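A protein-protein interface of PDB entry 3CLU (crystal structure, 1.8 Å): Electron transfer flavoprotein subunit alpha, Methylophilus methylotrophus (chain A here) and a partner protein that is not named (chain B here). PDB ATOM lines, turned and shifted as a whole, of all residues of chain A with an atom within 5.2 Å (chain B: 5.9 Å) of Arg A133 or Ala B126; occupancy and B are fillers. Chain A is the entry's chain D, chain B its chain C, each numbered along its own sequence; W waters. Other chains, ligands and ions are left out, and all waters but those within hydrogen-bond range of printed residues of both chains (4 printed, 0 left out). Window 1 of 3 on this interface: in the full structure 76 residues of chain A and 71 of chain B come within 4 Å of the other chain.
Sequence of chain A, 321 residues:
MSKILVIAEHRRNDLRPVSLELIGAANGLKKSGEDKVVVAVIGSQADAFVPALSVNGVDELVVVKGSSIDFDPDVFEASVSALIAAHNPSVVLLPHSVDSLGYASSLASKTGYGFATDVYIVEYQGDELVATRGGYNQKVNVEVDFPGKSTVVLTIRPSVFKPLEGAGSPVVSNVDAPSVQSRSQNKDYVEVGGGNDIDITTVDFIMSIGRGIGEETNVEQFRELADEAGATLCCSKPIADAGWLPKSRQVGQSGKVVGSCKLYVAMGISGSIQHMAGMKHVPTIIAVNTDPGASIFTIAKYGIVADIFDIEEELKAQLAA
Arg A133 touches just these residues of chain B: Gln B125 (2.9 Å), Ala B126 (3.0 Å) and Tyr B127 (3.5 Å).
Ala B126 touches one residue of chain A.
Of the printed residues of chain B, Thr A117 touches Tyr B127.
Of the printed residues of chain A, Asp B124 touches Gly A135.
Printed residues of chain A within 4 Å of Tyr B127: Thr A117 and Arg A133.
Printed residues of chain B within 4 Å of Gly A135: Asp B124 (3.7 Å) and Gln B125 (3.1 Å).
Of the printed residues of chain A, Gln B125 touches Arg A133 (2.9 Å) and Gly A135 (3.1 Å).
Val A119 touches none of the printed residues of chain B.
The nearest residue of chain B that does not touch Arg A133 is Ala B128 (5.6 Å).
The nearest residue of chain A that does not touch Ala B126 is Thr A117 (4.2 Å).
Water W3 lies within hydrogen-bond range of the side-chain carboxylate of Asp A118 (2.5 Å), the backbone carbonyl oxygen of Ala B126 (2.8 Å) and the guanidinium group of Arg A133 (3.3 Å).
Water W1 lies within hydrogen-bond range of NE2 of Gln B121, NE2 of His A96 and O of Ala B126.
Water W2 lies within hydrogen-bond range of the backbone carbonyl oxygen (O) of Gly A134 (2.8 Å) and the backbone carbonyl oxygen (O) of Gln B125 (2.9 Å).
Water W4 lies within hydrogen-bond range of O of Asp B124 (2.8 Å) and N of Gly A135 (3.4 Å).
Among the printed residues, pairs that only touch across the chains: Arg A133 with Tyr B127, Gly A135 with Asp B124 and Gly A135 with Gln B125.
O of Ala B126 sits at hydrogen-bond distance from NH2 of Arg A133, at 3.0 Å.
The side-chain hydroxyl (OG1) of Thr A117 is in hydrogen-bond range of the backbone carbonyl oxygen (O) of Tyr B127, at 2.7 Å.
O of Gln B125 is in hydrogen-bond range of NH1 of Arg A133 (2.9 Å).
The side-chain hydroxyl (OH) of Tyr A120 sits close to the backbone carbonyl oxygen (O) of Arg A133 (3.3 Å).
OG of Ser B122 sits at hydrogen-bond distance from OD1 of Asp B124 (3.2 Å).
The backbone carbonyl oxygen of Arg A133 sits at hydrogen-bond distance from the backbone NH of Val A142 (2.8 Å).
The guanidinium group (NE) of Arg A133 lies within hydrogen-bond range of the backbone carbonyl oxygen (O) of Thr A117 (2.8 Å).
N of Ala B126 lies within hydrogen-bond range of OG of Ser B122 (3.1 Å).
O of Val A140 sits at hydrogen-bond distance from N of Gly A135 (2.9 Å).
Of the 15 printed residues of chain A, 3 touch a printed residue of chain B.
Printed residues of chain A that touch a printed residue of chain B: Thr A117, Arg A133 and Gly A135.
Among the printed residues, 6 pairs touch across the chains.
Among the printed residues, no Asp or Glu carboxylate lies within 4 Å of a Lys or Arg side-chain nitrogen of the other chain.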
ATOM      1  N   HIS A  96       5.561  14.427  11.659  1.00  0.00           N
ATOM      2  CA  HIS A  96       5.360  15.139  12.944  1.00  0.00           C
ATOM      3  C   HIS A  96       5.095  14.104  14.051  1.00  0.00           C
ATOM      4  O   HIS A  96       3.964  13.904  14.513  1.00  0.00           O
ATOM      5  CB  HIS A  96       4.236  16.157  12.856  1.00  0.00           C
ATOM      6  CG  HIS A  96       4.226  17.145  13.984  1.00  0.00           C
ATOM      7  ND1 HIS A  96       5.263  18.022  14.198  1.00  0.00           N
ATOM      8  CD2 HIS A  96       3.328  17.366  14.979  1.00  0.00           C
ATOM      9  CE1 HIS A  96       4.989  18.772  15.253  1.00  0.00           C
ATOM     10  NE2 HIS A  96       3.832  18.384  15.756  1.00  0.00           N
ATOM     11  N   ALA A 116       8.627  24.534   8.965  1.00  0.00           N
ATOM     12  CA  ALA A 116       7.256  24.590   9.510  1.00  0.00           C
ATOM     13  C   ALA A 116       6.871  23.191   9.967  1.00  0.00           C
ATOM     14  O   ALA A 116       7.319  22.203   9.382  1.00  0.00           O
ATOM     15  CB  ALA A 116       6.301  25.082   8.526  1.00  0.00           C
ATOM     16  N   THR A 117       6.053  23.122  11.014  1.00  0.00           N
ATOM     17  CA  THR A 117       5.707  21.856  11.658  1.00  0.00           C
ATOM     18  C   THR A 117       4.226  21.523  11.593  1.00  0.00           C
ATOM     19  O   THR A 117       3.380  22.413  11.424  1.00  0.00           O
ATOM     20  CB  THR A 117       6.155  21.804  13.140  1.00  0.00           C
ATOM     21  OG1 THR A 117       5.444  22.770  13.926  1.00  0.00           O
ATOM     22  CG2 THR A 117       7.653  22.029  13.274  1.00  0.00           C
ATOM     23  N   ASP A 118       3.925  20.231  11.698  1.00  0.00           N
ATOM     24  CA  ASP A 118       2.545  19.757  11.760  1.00  0.00           C
ATOM     25  C   ASP A 118       1.711  20.298  10.586  1.00  0.00           C
ATOM     26  O   ASP A 118       0.590  20.730  10.782  1.00  0.00           O
ATOM     27  CB  ASP A 118       1.907  20.122  13.126  1.00  0.00           C
ATOM     28  CG  ASP A 118       0.615  19.355  13.400  1.00  0.00           C
ATOM     29  OD1 ASP A 118       0.435  18.273  12.816  1.00  0.00           O
ATOM     30  OD2 ASP A 118      -0.229  19.833  14.186  1.00  0.00           O
ATOM     31  N   VAL A 119       2.288  20.206   9.384  1.00  0.00           N
ATOM     32  CA  VAL A 119       1.738  20.729   8.152  1.00  0.00           C
ATOM     33  C   VAL A 119       0.746  19.733   7.591  1.00  0.00           C
ATOM     34  O   VAL A 119       1.055  18.556   7.519  1.00  0.00           O
ATOM     35  CB  VAL A 119       2.876  20.952   7.136  1.00  0.00           C
ATOM     36  CG1 VAL A 119       2.342  21.264   5.740  1.00  0.00           C
ATOM     37  CG2 VAL A 119       3.790  22.060   7.627  1.00  0.00           C
ATOM     38  N   TYR A 120      -0.437  20.203   7.186  1.00  0.00           N
ATOM     39  CA  TYR A 120      -1.432  19.300   6.615  1.00  0.00           C
ATOM     40  C   TYR A 120      -1.964  19.717   5.239  1.00  0.00           C
ATOM     41  O   TYR A 120      -2.859  19.049   4.670  1.00  0.00           O
ATOM     42  CB  TYR A 120      -2.564  19.083   7.600  1.00  0.00           C
ATOM     43  CG  TYR A 120      -3.136  20.314   8.199  1.00  0.00           C
ATOM     44  CD1 TYR A 120      -4.101  21.059   7.538  1.00  0.00           C
ATOM     45  CD2 TYR A 120      -2.739  20.737   9.459  1.00  0.00           C
ATOM     46  CE1 TYR A 120      -4.649  22.204   8.130  1.00  0.00           C
ATOM     47  CE2 TYR A 120      -3.282  21.843  10.036  1.00  0.00           C
ATOM     48  CZ  TYR A 120      -4.228  22.574   9.395  1.00  0.00           C
ATOM     49  OH  TYR A 120      -4.755  23.685  10.036  1.00  0.00           O
ATOM     50  N   ALA A 131       2.994  25.999   2.533  1.00  0.00           N
ATOM     51  CA  ALA A 131       2.587  25.036   3.535  1.00  0.00           C
ATOM     52  C   ALA A 131       1.503  25.659   4.408  1.00  0.00           C
ATOM     53  O   ALA A 131       1.531  26.857   4.701  1.00  0.00           O
ATOM     54  CB  ALA A 131       3.776  24.638   4.383  1.00  0.00           C
ATOM     55  N   THR A 132       0.530  24.836   4.797  1.00  0.00           N
ATOM     56  CA  THR A 132      -0.532  25.262   5.684  1.00  0.00           C
ATOM     57  C   THR A 132      -0.530  24.394   6.930  1.00  0.00           C
ATOM     58  O   THR A 132      -0.437  23.176   6.856  1.00  0.00           O
ATOM     59  CB  THR A 132      -1.897  25.164   5.033  1.00  0.00           C
ATOM     60  OG1 THR A 132      -1.873  25.871   3.772  1.00  0.00           O
ATOM     61  CG2 THR A 132      -2.975  25.756   5.962  1.00  0.00           C
ATOM     62  N   ARG A 133      -0.691  25.049   8.057  1.00  0.00           N
ATOM     63  CA  ARG A 133      -0.730  24.408   9.372  1.00  0.00           C
ATOM     64  C   ARG A 133      -1.834  25.090  10.194  1.00  0.00           C
ATOM     65  O   ARG A 133      -2.477  26.007   9.717  1.00  0.00           O
ATOM     66  CB  ARG A 133       0.649  24.532  10.034  1.00  0.00           C
ATOM     67  CG  ARG A 133       0.999  25.964  10.499  1.00  0.00           C
ATOM     68  CD  ARG A 133       2.388  26.092  11.076  1.00  0.00           C
ATOM     69  NE  ARG A 133       2.652  25.052  12.059  1.00  0.00           N
ATOM     70  CZ  ARG A 133       2.280  25.107  13.334  1.00  0.00           C
ATOM     71  NH1 ARG A 133       1.626  26.167  13.809  1.00  0.00           N
ATOM     72  NH2 ARG A 133       2.576  24.099  14.146  1.00  0.00           N
ATOM     73  N   GLY A 134      -2.074  24.647  11.421  1.00  0.00           N
ATOM     74  CA  GLY A 134      -3.126  25.261  12.235  1.00  0.00           C
ATOM     75  C   GLY A 134      -2.651  26.450  13.028  1.00  0.00           C
ATOM     76  O   GLY A 134      -1.454  26.632  13.236  1.00  0.00           O
ATOM     77  N   GLY A 135      -3.594  27.257  13.488  1.00  0.00           N
ATOM     78  CA  GLY A 135      -3.317  28.264  14.511  1.00  0.00           C
ATOM     79  C   GLY A 135      -4.424  28.275  15.568  1.00  0.00           C
ATOM     80  O   GLY A 135      -5.555  27.837  15.306  1.00  0.00           O
ATOM     81  N   VAL A 140      -7.880  28.209  13.190  1.00  0.00           N
ATOM     82  CA  VAL A 140      -7.572  28.801  11.910  1.00  0.00           C
ATOM     83  C   VAL A 140      -6.585  27.951  11.125  1.00  0.00           C
ATOM     84  O   VAL A 140      -5.903  27.093  11.686  1.00  0.00           O
ATOM     85  CB  VAL A 140      -7.025  30.233  12.026  1.00  0.00           C
ATOM     86  CG1 VAL A 140      -8.075  31.177  12.673  1.00  0.00           C
ATOM     87  CG2 VAL A 140      -5.702  30.262  12.736  1.00  0.00           C
ATOM     88  N   ASN A 141      -6.539  28.198   9.815  1.00  0.00           N
ATOM     89  CA  ASN A 141      -5.405  27.809   9.008  1.00  0.00           C
ATOM     90  C   ASN A 141      -4.415  28.961   8.883  1.00  0.00           C
ATOM     91  O   ASN A 141      -4.787  30.115   8.724  1.00  0.00           O
ATOM     92  CB  ASN A 141      -5.821  27.350   7.621  1.00  0.00           C
ATOM     93  CG  ASN A 141      -6.422  25.947   7.618  1.00  0.00           C
ATOM     94  OD1 ASN A 141      -6.551  25.297   8.663  1.00  0.00           O
ATOM     95  ND2 ASN A 141      -6.801  25.486   6.443  1.00  0.00           N
ATOM     96  N   VAL A 142      -3.143  28.614   9.007  1.00  0.00           N
ATOM     97  CA  VAL A 142      -2.069  29.551   8.801  1.00  0.00           C
ATOM     98  C   VAL A 142      -1.283  29.063   7.603  1.00  0.00           C
ATOM     99  O   VAL A 142      -0.688  27.981   7.634  1.00  0.00           O
ATOM    100  CB  VAL A 142      -1.144  29.642  10.038  1.00  0.00           C
ATOM    101  CG1 VAL A 142      -0.089  30.718   9.839  1.00  0.00           C
ATOM    102  CG2 VAL A 142      -1.961  29.947  11.309  1.00  0.00           C
ATOM    103  N   GLU A 143      -1.276  29.868   6.557  1.00  0.00           N
ATOM    104  CA  GLU A 143      -0.592  29.523   5.325  1.00  0.00           C
ATOM    105  C   GLU A 143       0.711  30.309   5.275  1.00  0.00           C
ATOM    106  O   GLU A 143       0.720  31.550   5.420  1.00  0.00           O
ATOM    107  CB  GLU A 143      -1.494  29.848   4.158  1.00  0.00           C
ATOM    108  CG  GLU A 143      -0.984  29.515   2.794  1.00  0.00           C
ATOM    109  CD  GLU A 143      -1.910  30.105   1.753  1.00  0.00           C
ATOM    110  OE1 GLU A 143      -2.976  29.517   1.525  1.00  0.00           O
ATOM    111  OE2 GLU A 143      -1.616  31.196   1.216  1.00  0.00           O
ATOM    112  N   GLN B 121       4.677  21.472  23.660  1.00  0.00           N
ATOM    113  CA  GLN B 121       4.160  22.376  22.690  1.00  0.00           C
ATOM    114  C   GLN B 121       3.300  23.440  23.355  1.00  0.00           C
ATOM    115  O   GLN B 121       3.019  23.378  24.552  1.00  0.00           O
ATOM    116  CB  GLN B 121       3.342  21.620  21.671  1.00  0.00           C
ATOM    117  CG  GLN B 121       2.082  21.047  22.195  1.00  0.00           C
ATOM    118  CD  GLN B 121       1.258  20.384  21.109  1.00  0.00           C
ATOM    119  OE1 GLN B 121       0.039  20.533  21.067  1.00  0.00           O
ATOM    120  NE2 GLN B 121       1.926  19.713  20.191  1.00  0.00           N
ATOM    121  N   SER B 122       2.905  24.437  22.560  1.00  0.00           N
ATOM    122  CA  SER B 122       2.016  25.494  22.994  1.00  0.00           C
ATOM    123  C   SER B 122       0.605  25.149  22.540  1.00  0.00           C
ATOM    124  O   SER B 122       0.403  24.601  21.445  1.00  0.00           O
ATOM    125  CB  SER B 122       2.416  26.879  22.427  1.00  0.00           C
ATOM    126  OG  SER B 122       2.578  26.845  21.018  1.00  0.00           O
ATOM    127  N   SER B 123      -0.365  25.467  23.390  1.00  0.00           N
ATOM    128  CA  SER B 123      -1.775  25.130  23.117  1.00  0.00           C
ATOM    129  C   SER B 123      -2.314  25.960  21.963  1.00  0.00           C
ATOM    130  O   SER B 123      -3.227  25.531  21.223  1.00  0.00           O
ATOM    131  CB  SER B 123      -2.622  25.361  24.366  1.00  0.00           C
ATOM    132  OG  SER B 123      -2.600  26.715  24.770  1.00  0.00           O
ATOM    133  N   ASP B 124      -1.761  27.151  21.784  1.00  0.00           N
ATOM    134  CA  ASP B 124      -2.203  27.975  20.684  1.00  0.00           C
ATOM    135  C   ASP B 124      -1.596  27.574  19.324  1.00  0.00           C
ATOM    136  O   ASP B 124      -2.318  27.119  18.436  1.00  0.00           O
ATOM    137  CB  ASP B 124      -2.052  29.466  20.970  1.00  0.00           C
ATOM    138  CG  ASP B 124      -0.654  29.886  21.458  1.00  0.00           C
ATOM    139  OD1 ASP B 124       0.355  29.143  21.356  1.00  0.00           O
ATOM    140  OD2 ASP B 124      -0.606  31.034  21.943  1.00  0.00           O
ATOM    141  N   GLN B 125      -0.281  27.685  19.159  1.00  0.00           N
ATOM    142  CA  GLN B 125       0.286  27.432  17.833  1.00  0.00           C
ATOM    143  C   GLN B 125       0.797  25.985  17.660  1.00  0.00           C
ATOM    144  O   GLN B 125       0.957  25.507  16.523  1.00  0.00           O
ATOM    145  CB  GLN B 125       1.340  28.497  17.483  1.00  0.00           C
ATOM    146  CG  GLN B 125       0.845  29.964  17.544  1.00  0.00           C
ATOM    147  CD  GLN B 125      -0.671  30.225  17.221  1.00  0.00           C
ATOM    148  OE1 GLN B 125      -1.291  29.553  16.417  1.00  0.00           O
ATOM    149  NE2 GLN B 125      -1.231  31.233  17.855  1.00  0.00           N
ATOM    150  N   ALA B 126       1.078  25.310  18.768  1.00  0.00           N
ATOM    151  CA  ALA B 126       1.406  23.904  18.750  1.00  0.00           C
ATOM    152  C   ALA B 126       2.557  23.665  17.730  1.00  0.00           C
ATOM    153  O   ALA B 126       2.448  22.827  16.828  1.00  0.00           O
ATOM    154  CB  ALA B 126       0.186  23.109  18.424  1.00  0.00           C
ATOM    155  N   TYR B 127       3.629  24.467  17.847  1.00  0.00           N
ATOM    156  CA  TYR B 127       4.812  24.320  16.978  1.00  0.00           C
ATOM    157  C   TYR B 127       5.577  23.071  17.369  1.00  0.00           C
ATOM    158  O   TYR B 127       6.185  22.401  16.517  1.00  0.00           O
ATOM    159  CB  TYR B 127       5.771  25.517  17.078  1.00  0.00           C
ATOM    160  CG  TYR B 127       5.199  26.858  16.655  1.00  0.00           C
ATOM    161  CD1 TYR B 127       5.227  27.935  17.531  1.00  0.00           C
ATOM    162  CD2 TYR B 127       4.687  27.060  15.370  1.00  0.00           C
ATOM    163  CE1 TYR B 127       4.744  29.168  17.178  1.00  0.00           C
ATOM    164  CE2 TYR B 127       4.194  28.290  14.996  1.00  0.00           C
ATOM    165  CZ  TYR B 127       4.218  29.347  15.912  1.00  0.00           C
ATOM    166  OH  TYR B 127       3.725  30.604  15.619  1.00  0.00           O
ATOM    167  N   ALA B 128       5.555  22.788  18.673  1.00  0.00           N
ATOM    168  CA  ALA B 128       6.380  21.707  19.259  1.00  0.00           C
ATOM    169  C   ALA B 128       7.854  21.817  18.757  1.00  0.00           C
ATOM    170  O   ALA B 128       8.450  20.821  18.273  1.00  0.00           O
ATOM    171  CB  ALA B 128       5.780  20.354  18.912  1.00  0.00           C
HETATM  172  O   HOH W   1       2.364  19.737  17.593  1.00  0.00           O
HETATM  173  O   HOH W   2      -1.171  24.345  14.884  1.00  0.00           O
HETATM  174  O   HOH W   3       0.224  22.056  15.249  1.00  0.00           O
HETATM  175  O   HOH W   4      -3.212  25.450  16.318  1.00  0.00           O
